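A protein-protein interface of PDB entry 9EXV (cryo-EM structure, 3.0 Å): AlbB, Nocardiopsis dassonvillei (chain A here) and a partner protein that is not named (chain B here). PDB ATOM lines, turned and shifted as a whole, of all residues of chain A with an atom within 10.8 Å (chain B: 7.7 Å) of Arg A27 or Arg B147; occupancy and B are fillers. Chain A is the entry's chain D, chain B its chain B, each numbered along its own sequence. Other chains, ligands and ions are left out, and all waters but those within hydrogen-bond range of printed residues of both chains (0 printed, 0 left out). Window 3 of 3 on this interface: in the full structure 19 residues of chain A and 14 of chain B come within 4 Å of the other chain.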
ATOM      1  N   ALA A  19     -15.934 -25.640 -18.246  1.00  0.00           N
ATOM      2  CA  ALA A  19     -16.369 -24.328 -17.779  1.00  0.00           C
ATOM      3  C   ALA A  19     -17.420 -23.741 -18.707  1.00  0.00           C
ATOM      4  O   ALA A  19     -18.387 -23.122 -18.252  1.00  0.00           O
ATOM      5  CB  ALA A  19     -15.170 -23.389 -17.660  1.00  0.00           C
ATOM      6  N   ALA A  20     -17.244 -23.922 -20.017  1.00  0.00           N
ATOM      7  CA  ALA A  20     -18.265 -23.477 -20.956  1.00  0.00           C
ATOM      8  C   ALA A  20     -19.582 -24.197 -20.712  1.00  0.00           C
ATOM      9  O   ALA A  20     -20.652 -23.582 -20.765  1.00  0.00           O
ATOM     10  CB  ALA A  20     -17.795 -23.692 -22.391  1.00  0.00           C
ATOM     11  N   TYR A  21     -19.527 -25.504 -20.442  1.00  0.00           N
ATOM     12  CA  TYR A  21     -20.751 -26.237 -20.138  1.00  0.00           C
ATOM     13  C   TYR A  21     -21.416 -25.707 -18.876  1.00  0.00           C
ATOM     14  O   TYR A  21     -22.643 -25.572 -18.823  1.00  0.00           O
ATOM     15  CB  TYR A  21     -20.470 -27.730 -19.989  1.00  0.00           C
ATOM     16  CG  TYR A  21     -21.538 -28.437 -19.184  1.00  0.00           C
ATOM     17  CD1 TYR A  21     -22.784 -28.709 -19.735  1.00  0.00           C
ATOM     18  CD2 TYR A  21     -21.306 -28.820 -17.870  1.00  0.00           C
ATOM     19  CE1 TYR A  21     -23.766 -29.347 -19.001  1.00  0.00           C
ATOM     20  CE2 TYR A  21     -22.282 -29.458 -17.129  1.00  0.00           C
ATOM     21  CZ  TYR A  21     -23.509 -29.719 -17.699  1.00  0.00           C
ATOM     22  OH  TYR A  21     -24.482 -30.353 -16.964  1.00  0.00           O
ATOM     23  N   LEU A  22     -20.624 -25.427 -17.837  1.00  0.00           N
ATOM     24  CA  LEU A  22     -21.196 -24.905 -16.601  1.00  0.00           C
ATOM     25  C   LEU A  22     -21.849 -23.550 -16.824  1.00  0.00           C
ATOM     26  O   LEU A  22     -22.935 -23.280 -16.298  1.00  0.00           O
ATOM     27  CB  LEU A  22     -20.119 -24.817 -15.520  1.00  0.00           C
ATOM     28  CG  LEU A  22     -19.852 -26.119 -14.763  1.00  0.00           C
ATOM     29  CD1 LEU A  22     -18.544 -26.043 -13.998  1.00  0.00           C
ATOM     30  CD2 LEU A  22     -21.005 -26.426 -13.819  1.00  0.00           C
ATOM     31  N   LEU A  23     -21.203 -22.683 -17.604  1.00  0.00           N
ATOM     32  CA  LEU A  23     -21.795 -21.388 -17.920  1.00  0.00           C
ATOM     33  C   LEU A  23     -23.086 -21.542 -18.709  1.00  0.00           C
ATOM     34  O   LEU A  23     -24.071 -20.842 -18.449  1.00  0.00           O
ATOM     35  CB  LEU A  23     -20.800 -20.545 -18.706  1.00  0.00           C
ATOM     36  CG  LEU A  23     -19.846 -19.733 -17.853  1.00  0.00           C
ATOM     37  CD1 LEU A  23     -18.709 -19.242 -18.726  1.00  0.00           C
ATOM     38  CD2 LEU A  23     -20.619 -18.586 -17.216  1.00  0.00           C
ATOM     39  N   SER A  24     -23.090 -22.442 -19.690  1.00  0.00           N
ATOM     40  CA  SER A  24     -24.300 -22.674 -20.466  1.00  0.00           C
ATOM     41  C   SER A  24     -25.417 -23.205 -19.580  1.00  0.00           C
ATOM     42  O   SER A  24     -26.576 -22.805 -19.724  1.00  0.00           O
ATOM     43  CB  SER A  24     -24.008 -23.639 -21.612  1.00  0.00           C
ATOM     44  OG  SER A  24     -25.161 -23.841 -22.404  1.00  0.00           O
ATOM     45  N   SER A  25     -25.084 -24.100 -18.647  1.00  0.00           N
ATOM     46  CA  SER A  25     -26.086 -24.590 -17.705  1.00  0.00           C
ATOM     47  C   SER A  25     -26.619 -23.461 -16.834  1.00  0.00           C
ATOM     48  O   SER A  25     -27.821 -23.395 -16.558  1.00  0.00           O
ATOM     49  CB  SER A  25     -25.490 -25.698 -16.839  1.00  0.00           C
ATOM     50  OG  SER A  25     -25.127 -26.820 -17.623  1.00  0.00           O
ATOM     51  N   GLY A  26     -25.735 -22.569 -16.385  1.00  0.00           N
ATOM     52  CA  GLY A  26     -26.187 -21.437 -15.597  1.00  0.00           C
ATOM     53  C   GLY A  26     -27.164 -20.562 -16.357  1.00  0.00           C
ATOM     54  O   GLY A  26     -28.211 -20.179 -15.831  1.00  0.00           O
ATOM     55  N   ARG A  27     -26.843 -20.244 -17.613  1.00  0.00           N
ATOM     56  CA  ARG A  27     -27.774 -19.464 -18.418  1.00  0.00           C
ATOM     57  C   ARG A  27     -29.068 -20.229 -18.652  1.00  0.00           C
ATOM     58  O   ARG A  27     -30.160 -19.647 -18.611  1.00  0.00           O
ATOM     59  CB  ARG A  27     -27.135 -19.075 -19.752  1.00  0.00           C
ATOM     60  CG  ARG A  27     -28.079 -18.312 -20.685  1.00  0.00           C
ATOM     61  CD  ARG A  27     -28.748 -17.136 -19.974  1.00  0.00           C
ATOM     62  NE  ARG A  27     -29.595 -16.353 -20.867  1.00  0.00           N
ATOM     63  CZ  ARG A  27     -30.849 -16.653 -21.172  1.00  0.00           C
ATOM     64  NH1 ARG A  27     -31.446 -17.720 -20.669  1.00  0.00           N
ATOM     65  NH2 ARG A  27     -31.520 -15.865 -22.008  1.00  0.00           N
ATOM     66  N   GLY A  28     -28.965 -21.536 -18.897  1.00  0.00           N
ATOM     67  CA  GLY A  28     -30.151 -22.319 -19.196  1.00  0.00           C
ATOM     68  C   GLY A  28     -31.111 -22.412 -18.026  1.00  0.00           C
ATOM     69  O   GLY A  28     -32.330 -22.381 -18.212  1.00  0.00           O
ATOM     70  N   LEU A  29     -30.579 -22.503 -16.804  1.00  0.00           N
ATOM     71  CA  LEU A  29     -31.430 -22.699 -15.635  1.00  0.00           C
ATOM     72  C   LEU A  29     -32.414 -21.554 -15.430  1.00  0.00           C
ATOM     73  O   LEU A  29     -33.396 -21.719 -14.700  1.00  0.00           O
ATOM     74  CB  LEU A  29     -30.570 -22.887 -14.383  1.00  0.00           C
ATOM     75  CG  LEU A  29     -29.845 -24.231 -14.264  1.00  0.00           C
ATOM     76  CD1 LEU A  29     -28.907 -24.243 -13.066  1.00  0.00           C
ATOM     77  CD2 LEU A  29     -30.838 -25.379 -14.177  1.00  0.00           C
ATOM     78  N   LEU A  30     -32.177 -20.401 -16.059  1.00  0.00           N
ATOM     79  CA  LEU A  30     -33.120 -19.289 -16.000  1.00  0.00           C
ATOM     80  C   LEU A  30     -34.384 -19.548 -16.808  1.00  0.00           C
ATOM     81  O   LEU A  30     -35.301 -18.721 -16.777  1.00  0.00           O
ATOM     82  CB  LEU A  30     -32.442 -18.009 -16.485  1.00  0.00           C
ATOM     83  CG  LEU A  30     -31.083 -17.718 -15.848  1.00  0.00           C
ATOM     84  CD1 LEU A  30     -30.503 -16.421 -16.374  1.00  0.00           C
ATOM     85  CD2 LEU A  30     -31.210 -17.669 -14.340  1.00  0.00           C
ATOM     86  N   ASP A  31     -34.439 -20.659 -17.542  1.00  0.00           N
ATOM     87  CA  ASP A  31     -35.624 -21.075 -18.283  1.00  0.00           C
ATOM     88  C   ASP A  31     -36.071 -22.495 -17.972  1.00  0.00           C
ATOM     89  O   ASP A  31     -37.230 -22.828 -18.244  1.00  0.00           O
ATOM     90  CB  ASP A  31     -35.381 -20.959 -19.794  1.00  0.00           C
ATOM     91  CG  ASP A  31     -35.228 -19.525 -20.256  1.00  0.00           C
ATOM     92  OD1 ASP A  31     -35.867 -18.634 -19.658  1.00  0.00           O
ATOM     93  OD2 ASP A  31     -34.473 -19.286 -21.222  1.00  0.00           O
ATOM     94  N   GLU A  32     -35.200 -23.340 -17.421  1.00  0.00           N
ATOM     95  CA  GLU A  32     -35.545 -24.717 -17.121  1.00  0.00           C
ATOM     96  C   GLU A  32     -36.456 -24.781 -15.898  1.00  0.00           C
ATOM     97  O   GLU A  32     -36.536 -23.823 -15.126  1.00  0.00           O
ATOM     98  CB  GLU A  32     -34.279 -25.539 -16.876  1.00  0.00           C
ATOM     99  CG  GLU A  32     -33.168 -25.338 -17.891  1.00  0.00           C
ATOM    100  CD  GLU A  32     -33.428 -26.032 -19.211  1.00  0.00           C
ATOM    101  OE1 GLU A  32     -34.493 -26.665 -19.360  1.00  0.00           O
ATOM    102  OE2 GLU A  32     -32.556 -25.946 -20.101  1.00  0.00           O
ATOM    103  N   PRO A  33     -37.154 -25.907 -15.692  1.00  0.00           N
ATOM    104  CA  PRO A  33     -38.006 -26.021 -14.500  1.00  0.00           C
ATOM    105  C   PRO A  33     -37.204 -25.958 -13.209  1.00  0.00           C
ATOM    106  O   PRO A  33     -35.972 -25.884 -13.232  1.00  0.00           O
ATOM    107  CB  PRO A  33     -38.687 -27.385 -14.680  1.00  0.00           C
ATOM    108  CG  PRO A  33     -37.808 -28.136 -15.612  1.00  0.00           C
ATOM    109  CD  PRO A  33     -37.235 -27.112 -16.539  1.00  0.00           C
ATOM    110  N   ARG A  34     -37.905 -25.981 -12.073  1.00  0.00           N
ATOM    111  CA  ARG A  34     -37.253 -25.753 -10.789  1.00  0.00           C
ATOM    112  C   ARG A  34     -36.252 -26.847 -10.443  1.00  0.00           C
ATOM    113  O   ARG A  34     -35.251 -26.577  -9.772  1.00  0.00           O
ATOM    114  CB  ARG A  34     -38.300 -25.640  -9.680  1.00  0.00           C
ATOM    115  CG  ARG A  34     -39.477 -24.723  -9.986  1.00  0.00           C
ATOM    116  CD  ARG A  34     -39.043 -23.280 -10.190  1.00  0.00           C
ATOM    117  NE  ARG A  34     -38.612 -23.025 -11.559  1.00  0.00           N
ATOM    118  CZ  ARG A  34     -39.434 -22.802 -12.575  1.00  0.00           C
ATOM    119  NH1 ARG A  34     -40.747 -22.809 -12.415  1.00  0.00           N
ATOM    120  NH2 ARG A  34     -38.926 -22.569 -13.782  1.00  0.00           N
ATOM    121  N   TYR A  36     -34.131 -28.727 -12.153  1.00  0.00           N
ATOM    122  CA  TYR A  36     -32.890 -28.960 -12.883  1.00  0.00           C
ATOM    123  C   TYR A  36     -31.674 -28.338 -12.209  1.00  0.00           C
ATOM    124  O   TYR A  36     -30.547 -28.622 -12.627  1.00  0.00           O
ATOM    125  CB  TYR A  36     -33.012 -28.446 -14.318  1.00  0.00           C
ATOM    126  CG  TYR A  36     -33.797 -29.371 -15.226  1.00  0.00           C
ATOM    127  CD1 TYR A  36     -34.500 -30.452 -14.707  1.00  0.00           C
ATOM    128  CD2 TYR A  36     -33.821 -29.175 -16.600  1.00  0.00           C
ATOM    129  CE1 TYR A  36     -35.212 -31.302 -15.525  1.00  0.00           C
ATOM    130  CE2 TYR A  36     -34.532 -30.024 -17.429  1.00  0.00           C
ATOM    131  CZ  TYR A  36     -35.225 -31.086 -16.885  1.00  0.00           C
ATOM    132  OH  TYR A  36     -35.934 -31.937 -17.698  1.00  0.00           O
ATOM    133  N   GLY A  37     -31.868 -27.517 -11.174  1.00  0.00           N
ATOM    134  CA  GLY A  37     -30.725 -26.986 -10.453  1.00  0.00           C
ATOM    135  C   GLY A  37     -29.826 -28.081  -9.912  1.00  0.00           C
ATOM    136  O   GLY A  37     -28.599 -27.989  -9.997  1.00  0.00           O
ATOM    137  N   ARG A  40     -28.400 -30.521 -13.165  1.00  0.00           N
ATOM    138  CA  ARG A  40     -27.239 -30.000 -13.877  1.00  0.00           C
ATOM    139  C   ARG A  40     -25.982 -30.101 -13.024  1.00  0.00           C
ATOM    140  O   ARG A  40     -24.895 -30.385 -13.539  1.00  0.00           O
ATOM    141  CB  ARG A  40     -27.495 -28.562 -14.316  1.00  0.00           C
ATOM    142  CG  ARG A  40     -28.600 -28.441 -15.352  1.00  0.00           C
ATOM    143  CD  ARG A  40     -28.179 -29.031 -16.690  1.00  0.00           C
ATOM    144  NE  ARG A  40     -29.324 -29.258 -17.566  1.00  0.00           N
ATOM    145  CZ  ARG A  40     -29.940 -28.308 -18.255  1.00  0.00           C
ATOM    146  NH1 ARG A  40     -29.552 -27.044 -18.191  1.00  0.00           N
ATOM    147  NH2 ARG A  40     -30.974 -28.632 -19.025  1.00  0.00           N
ATOM    148  N   LEU B  77     -19.751 -28.422 -29.509  1.00  0.00           N
ATOM    149  CA  LEU B  77     -21.209 -28.447 -29.454  1.00  0.00           C
ATOM    150  C   LEU B  77     -21.703 -29.061 -28.152  1.00  0.00           C
ATOM    151  O   LEU B  77     -22.668 -28.574 -27.558  1.00  0.00           O
ATOM    152  CB  LEU B  77     -21.766 -29.202 -30.657  1.00  0.00           C
ATOM    153  CG  LEU B  77     -21.908 -28.352 -31.919  1.00  0.00           C
ATOM    154  CD1 LEU B  77     -22.019 -29.224 -33.152  1.00  0.00           C
ATOM    155  CD2 LEU B  77     -23.117 -27.438 -31.802  1.00  0.00           C
ATOM    156  N   ALA B  79     -20.104 -29.014 -25.301  1.00  0.00           N
ATOM    157  CA  ALA B  79     -19.843 -28.026 -24.261  1.00  0.00           C
ATOM    158  C   ALA B  79     -20.898 -26.927 -24.270  1.00  0.00           C
ATOM    159  O   ALA B  79     -21.333 -26.465 -23.212  1.00  0.00           O
ATOM    160  CB  ALA B  79     -18.448 -27.432 -24.437  1.00  0.00           C
ATOM    161  N   PHE B  80     -21.329 -26.502 -25.454  1.00  0.00           N
ATOM    162  CA  PHE B  80     -22.287 -25.416 -25.583  1.00  0.00           C
ATOM    163  C   PHE B  80     -23.729 -25.891 -25.690  1.00  0.00           C
ATOM    164  O   PHE B  80     -24.623 -25.069 -25.907  1.00  0.00           O
ATOM    165  CB  PHE B  80     -21.929 -24.537 -26.780  1.00  0.00           C
ATOM    166  CG  PHE B  80     -20.873 -23.537 -26.468  1.00  0.00           C
ATOM    167  CD1 PHE B  80     -21.116 -22.556 -25.527  1.00  0.00           C
ATOM    168  CD2 PHE B  80     -19.634 -23.590 -27.077  1.00  0.00           C
ATOM    169  CE1 PHE B  80     -20.158 -21.639 -25.209  1.00  0.00           C
ATOM    170  CE2 PHE B  80     -18.669 -22.668 -26.761  1.00  0.00           C
ATOM    171  CZ  PHE B  80     -18.937 -21.706 -25.817  1.00  0.00           C
ATOM    172  N   SER B  81     -23.974 -27.190 -25.542  1.00  0.00           N
ATOM    173  CA  SER B  81     -25.326 -27.747 -25.535  1.00  0.00           C
ATOM    174  C   SER B  81     -25.486 -28.594 -24.282  1.00  0.00           C
ATOM    175  O   SER B  81     -25.140 -29.783 -24.280  1.00  0.00           O
ATOM    176  CB  SER B  81     -25.597 -28.563 -26.798  1.00  0.00           C
ATOM    177  OG  SER B  81     -26.904 -29.100 -26.785  1.00  0.00           O
ATOM    178  N   PRO B  82     -26.001 -28.018 -23.192  1.00  0.00           N
ATOM    179  CA  PRO B  82     -26.167 -28.807 -21.961  1.00  0.00           C
ATOM    180  C   PRO B  82     -27.109 -29.985 -22.119  1.00  0.00           C
ATOM    181  O   PRO B  82     -27.029 -30.930 -21.325  1.00  0.00           O
ATOM    182  CB  PRO B  82     -26.708 -27.784 -20.954  1.00  0.00           C
ATOM    183  CG  PRO B  82     -27.316 -26.711 -21.785  1.00  0.00           C
ATOM    184  CD  PRO B  82     -26.477 -26.633 -23.027  1.00  0.00           C
ATOM    185  N   GLY B  83     -27.997 -29.961 -23.113  1.00  0.00           N
ATOM    186  CA  GLY B  83     -28.886 -31.093 -23.319  1.00  0.00           C
ATOM    187  C   GLY B  83     -28.137 -32.374 -23.626  1.00  0.00           C
ATOM    188  O   GLY B  83     -28.538 -33.459 -23.197  1.00  0.00           O
ATOM    189  N   GLY B 144     -33.486 -29.660 -27.009  1.00  0.00           N
ATOM    190  CA  GLY B 144     -33.789 -28.286 -27.349  1.00  0.00           C
ATOM    191  C   GLY B 144     -33.278 -27.303 -26.318  1.00  0.00           C
ATOM    192  O   GLY B 144     -33.457 -26.091 -26.464  1.00  0.00           O
ATOM    193  N   SER B 145     -32.636 -27.809 -25.267  1.00  0.00           N
ATOM    194  CA  SER B 145     -32.113 -26.964 -24.194  1.00  0.00           C
ATOM    195  C   SER B 145     -30.651 -26.664 -24.496  1.00  0.00           C
ATOM    196  O   SER B 145     -29.743 -27.393 -24.091  1.00  0.00           O
ATOM    197  CB  SER B 145     -32.287 -27.640 -22.840  1.00  0.00           C
ATOM    198  OG  SER B 145     -31.441 -28.771 -22.710  1.00  0.00           O
ATOM    199  N   PHE B 146     -30.415 -25.577 -25.224  1.00  0.00           N
ATOM    200  CA  PHE B 146     -29.058 -25.184 -25.575  1.00  0.00           C
ATOM    201  C   PHE B 146     -29.028 -23.690 -25.852  1.00  0.00           C
ATOM    202  O   PHE B 146     -30.062 -23.058 -26.083  1.00  0.00           O
ATOM    203  CB  PHE B 146     -28.544 -25.963 -26.789  1.00  0.00           C
ATOM    204  CG  PHE B 146     -29.285 -25.660 -28.055  1.00  0.00           C
ATOM    205  CD1 PHE B 146     -30.535 -26.207 -28.288  1.00  0.00           C
ATOM    206  CD2 PHE B 146     -28.735 -24.826 -29.013  1.00  0.00           C
ATOM    207  CE1 PHE B 146     -31.222 -25.927 -29.451  1.00  0.00           C
ATOM    208  CE2 PHE B 146     -29.418 -24.544 -30.179  1.00  0.00           C
ATOM    209  CZ  PHE B 146     -30.663 -25.095 -30.398  1.00  0.00           C
ATOM    210  N   ARG B 147     -27.818 -23.136 -25.830  1.00  0.00           N
ATOM    211  CA  ARG B 147     -27.602 -21.725 -26.123  1.00  0.00           C
ATOM    212  C   ARG B 147     -27.590 -21.534 -27.632  1.00  0.00           C
ATOM    213  O   ARG B 147     -26.668 -21.995 -28.313  1.00  0.00           O
ATOM    214  CB  ARG B 147     -26.297 -21.247 -25.494  1.00  0.00           C
ATOM    215  CG  ARG B 147     -26.187 -21.503 -24.003  1.00  0.00           C
ATOM    216  CD  ARG B 147     -27.134 -20.631 -23.198  1.00  0.00           C
ATOM    217  NE  ARG B 147     -28.508 -21.117 -23.228  1.00  0.00           N
ATOM    218  CZ  ARG B 147     -28.937 -22.188 -22.577  1.00  0.00           C
ATOM    219  NH1 ARG B 147     -28.117 -22.927 -21.853  1.00  0.00           N
ATOM    220  NH2 ARG B 147     -30.218 -22.529 -22.657  1.00  0.00           N
ATOM    221  N   ARG B 148     -28.613 -20.857 -28.159  1.00  0.00           N
ATOM    222  CA  ARG B 148     -28.714 -20.687 -29.606  1.00  0.00           C
ATOM    223  C   ARG B 148     -27.548 -19.881 -30.158  1.00  0.00           C
ATOM    224  O   ARG B 148     -27.054 -20.170 -31.253  1.00  0.00           O
ATOM    225  CB  ARG B 148     -30.037 -20.022 -29.978  1.00  0.00           C
ATOM    226  CG  ARG B 148     -31.195 -20.986 -30.145  1.00  0.00           C
ATOM    227  CD  ARG B 148     -31.883 -21.238 -28.822  1.00  0.00           C
ATOM    228  NE  ARG B 148     -32.821 -22.351 -28.892  1.00  0.00           N
ATOM    229  CZ  ARG B 148     -33.296 -22.992 -27.834  1.00  0.00           C
ATOM    230  NH1 ARG B 148     -32.919 -22.675 -26.607  1.00  0.00           N
ATOM    231  NH2 ARG B 148     -34.171 -23.977 -28.013  1.00  0.00           N
ATOM    232  N   GLY B 149     -27.108 -18.860 -29.433  1.00  0.00           N
ATOM    233  CA  GLY B 149     -26.070 -17.981 -29.922  1.00  0.00           C
ATOM    234  C   GLY B 149     -24.772 -18.703 -30.219  1.00  0.00           C
ATOM    235  O   GLY B 149     -24.332 -18.790 -31.370  1.00  0.00           O
ATOM    236  N   PRO B 150     -24.121 -19.221 -29.174  1.00  0.00           N
ATOM    237  CA  PRO B 150     -22.853 -19.935 -29.395  1.00  0.00           C
ATOM    238  C   PRO B 150     -22.986 -21.132 -30.321  1.00  0.00           C
ATOM    239  O   PRO B 150     -22.086 -21.378 -31.131  1.00  0.00           O
ATOM    240  CB  PRO B 150     -22.439 -20.352 -27.976  1.00  0.00           C
ATOM    241  CG  PRO B 150     -23.145 -19.394 -27.073  1.00  0.00           C
ATOM    242  CD  PRO B 150     -24.448 -19.093 -27.744  1.00  0.00           C
ATOM    243  N   VAL B 151     -24.090 -21.877 -30.234  1.00  0.00           N
ATOM    244  CA  VAL B 151     -24.271 -23.038 -31.105  1.00  0.00           C
ATOM    245  C   VAL B 151     -24.358 -22.604 -32.561  1.00  0.00           C
ATOM    246  O   VAL B 151     -23.751 -23.217 -33.447  1.00  0.00           O
ATOM    247  CB  VAL B 151     -25.510 -23.840 -30.669  1.00  0.00           C
ATOM    248  CG1 VAL B 151     -25.983 -24.753 -31.786  1.00  0.00           C
ATOM    249  CG2 VAL B 151     -25.200 -24.646 -29.416  1.00  0.00           C
ATOM    250  N   ARG B 152     -25.117 -21.539 -32.826  1.00  0.00           N
ATOM    251  CA  ARG B 152     -25.159 -20.962 -34.165  1.00  0.00           C
ATOM    252  C   ARG B 152     -23.766 -20.562 -34.627  1.00  0.00           C
ATOM    253  O   ARG B 152     -23.371 -20.838 -35.764  1.00  0.00           O
ATOM    254  CB  ARG B 152     -26.092 -19.750 -34.171  1.00  0.00           C
ATOM    255  CG  ARG B 152     -25.801 -18.696 -35.231  1.00  0.00           C
ATOM    256  CD  ARG B 152     -26.536 -17.405 -34.912  1.00  0.00           C
ATOM    257  NE  ARG B 152     -27.954 -17.649 -34.687  1.00  0.00           N
ATOM    258  CZ  ARG B 152     -28.824 -17.901 -35.654  1.00  0.00           C
ATOM    259  NH1 ARG B 152     -28.452 -17.948 -36.922  1.00  0.00           N
ATOM    260  NH2 ARG B 152     -30.098 -18.116 -35.341  1.00  0.00           N
ATOM    261  N   ARG B 153     -23.006 -19.912 -33.747  1.00  0.00           N
ATOM    262  CA  ARG B 153     -21.680 -19.450 -34.125  1.00  0.00           C
ATOM    263  C   ARG B 153     -20.777 -20.615 -34.505  1.00  0.00           C
ATOM    264  O   ARG B 153     -20.036 -20.537 -35.494  1.00  0.00           O
ATOM    265  CB  ARG B 153     -21.075 -18.639 -32.990  1.00  0.00           C
ATOM    266  CG  ARG B 153     -21.796 -17.330 -32.703  1.00  0.00           C
ATOM    267  CD  ARG B 153     -21.158 -16.569 -31.555  1.00  0.00           C
ATOM    268  NE  ARG B 153     -19.800 -16.145 -31.875  1.00  0.00           N
ATOM    269  CZ  ARG B 153     -18.715 -16.885 -31.683  1.00  0.00           C
ATOM    270  NH1 ARG B 153     -18.783 -18.086 -31.130  1.00  0.00           N
ATOM    271  NH2 ARG B 153     -17.534 -16.413 -32.065  1.00  0.00           N
ATOM    272  N   LEU B 154     -20.823 -21.705 -33.735  1.00  0.00           N
ATOM    273  CA  LEU B 154     -20.032 -22.880 -34.083  1.00  0.00           C
ATOM    274  C   LEU B 154     -20.501 -23.493 -35.395  1.00  0.00           C
ATOM    275  O   LEU B 154     -19.680 -23.875 -36.236  1.00  0.00           O
ATOM    276  CB  LEU B 154     -20.098 -23.914 -32.960  1.00  0.00           C
ATOM    277  CG  LEU B 154     -19.794 -23.419 -31.546  1.00  0.00           C
ATOM    278  CD1 LEU B 154     -19.958 -24.543 -30.535  1.00  0.00           C
ATOM    279  CD2 LEU B 154     -18.408 -22.796 -31.459  1.00  0.00           C
ATOM    280  N   PRO B 163     -31.305 -22.345 -35.340  1.00  0.00           N
ATOM    281  CA  PRO B 163     -31.279 -23.711 -34.804  1.00  0.00           C
ATOM    282  C   PRO B 163     -32.352 -23.918 -33.746  1.00  0.00           C
ATOM    283  O   PRO B 163     -32.615 -23.044 -32.917  1.00  0.00           O
ATOM    284  CB  PRO B 163     -29.868 -23.837 -34.217  1.00  0.00           C
ATOM    285  CG  PRO B 163     -29.415 -22.439 -33.987  1.00  0.00           C
ATOM    286  CD  PRO B 163     -30.057 -21.614 -35.060  1.00  0.00           C
ATOM    287  N   LEU B 166     -30.903 -30.120 -31.504  1.00  0.00           N
ATOM    288  CA  LEU B 166     -29.636 -30.827 -31.629  1.00  0.00           C
ATOM    289  C   LEU B 166     -29.869 -32.297 -31.317  1.00  0.00           C
ATOM    290  O   LEU B 166     -30.409 -32.630 -30.257  1.00  0.00           O
ATOM    291  CB  LEU B 166     -28.577 -30.244 -30.692  1.00  0.00           C
ATOM    292  CG  LEU B 166     -27.778 -29.076 -31.270  1.00  0.00           C
ATOM    293  CD1 LEU B 166     -28.663 -27.855 -31.451  1.00  0.00           C
ATOM    294  CD2 LEU B 166     -26.578 -28.752 -30.395  1.00  0.00           C
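Of chain B, only Arg B147 (3.5 Å) comes within 4 Å of Arg A27. Of chain A, only Ser A24, Arg A27 and Gly A28 come within 4 Å of Arg B147. No residue of chain B comes within 4 Å of Gly A26. Of chain B, only Arg B147 comes within 4 Å of Gly A28. No residue of chain A comes within 4 Å of Gly B149. Pro B150 touches none of the printed residues of chain A. No residue of chain A comes within 4 Å of Val B151. Of the printed residues of chain B, Glu A32 touches Ser B145. Of the printed residues of chain A, Phe B80 touches Ser A24. Of the printed residues of chain B, Arg A40 touches Ser B145 (3.7 Å). Leu A30 touches none of the printed residues of chain B. Pro A33 touches none of the printed residues of chain B. The nearest residue of chain A that does not touch Arg B147 is Ser A25 (4.6 Å).
Among the printed residues, merely in contact across the chains: Ala A20 with Ala B79 (3.8 Å), Tyr A21 with Pro B82 (3.8 Å), Ser A24 with Phe B80 (3.8 Å), Ser A24 with Pro B82 (3.1 Å), Ser A25 with Pro B82 (3.8 Å), Arg A27 with Arg B147 (3.5 Å), Glu A32 with Ser B145 (3.2 Å) and Arg A40 with Ser B145 (3.7 Å).
The backbone NH (N) of Gly B83 lies within hydrogen-bond range of the backbone carbonyl oxygen (O) of Ser B145 (3.3 Å). O of Tyr A21 is in hydrogen-bond range of OG of Ser A25 (3.0 Å). O of Arg A40 lies within hydrogen-bond range of OH of Tyr A21 (3.4 Å). The guanidinium group (NH1) of Arg A27 lies within salt-bridge range of the side-chain carboxylate (OD2) of Asp A31. The guanidinium group (NH2) of Arg A34 lies within hydrogen-bond range of the backbone carbonyl oxygen (O) of Glu A32, 3.0 Å away. The side-chain carboxylate (OE2) of Glu A32 is in salt-bridge range of the guanidinium group (NH2) of Arg A40.
Of the 19 printed residues of chain B, 5 touch a printed residue of chain A. Among the printed residues, 11 pairs touch across the chains. Among the printed residues, no Asp or Glu carboxylate lies within 4 Å of a Lys or Arg side-chain nitrogen of the other chain.
O of Ala B79 lies close to N of Tyr A21. NH1 of Arg B147 is in hydrogen-bond range of O of Ser A24 (2.6 Å). NH1 of Arg B147 sits close to N of Gly A28 (3.4 Å).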
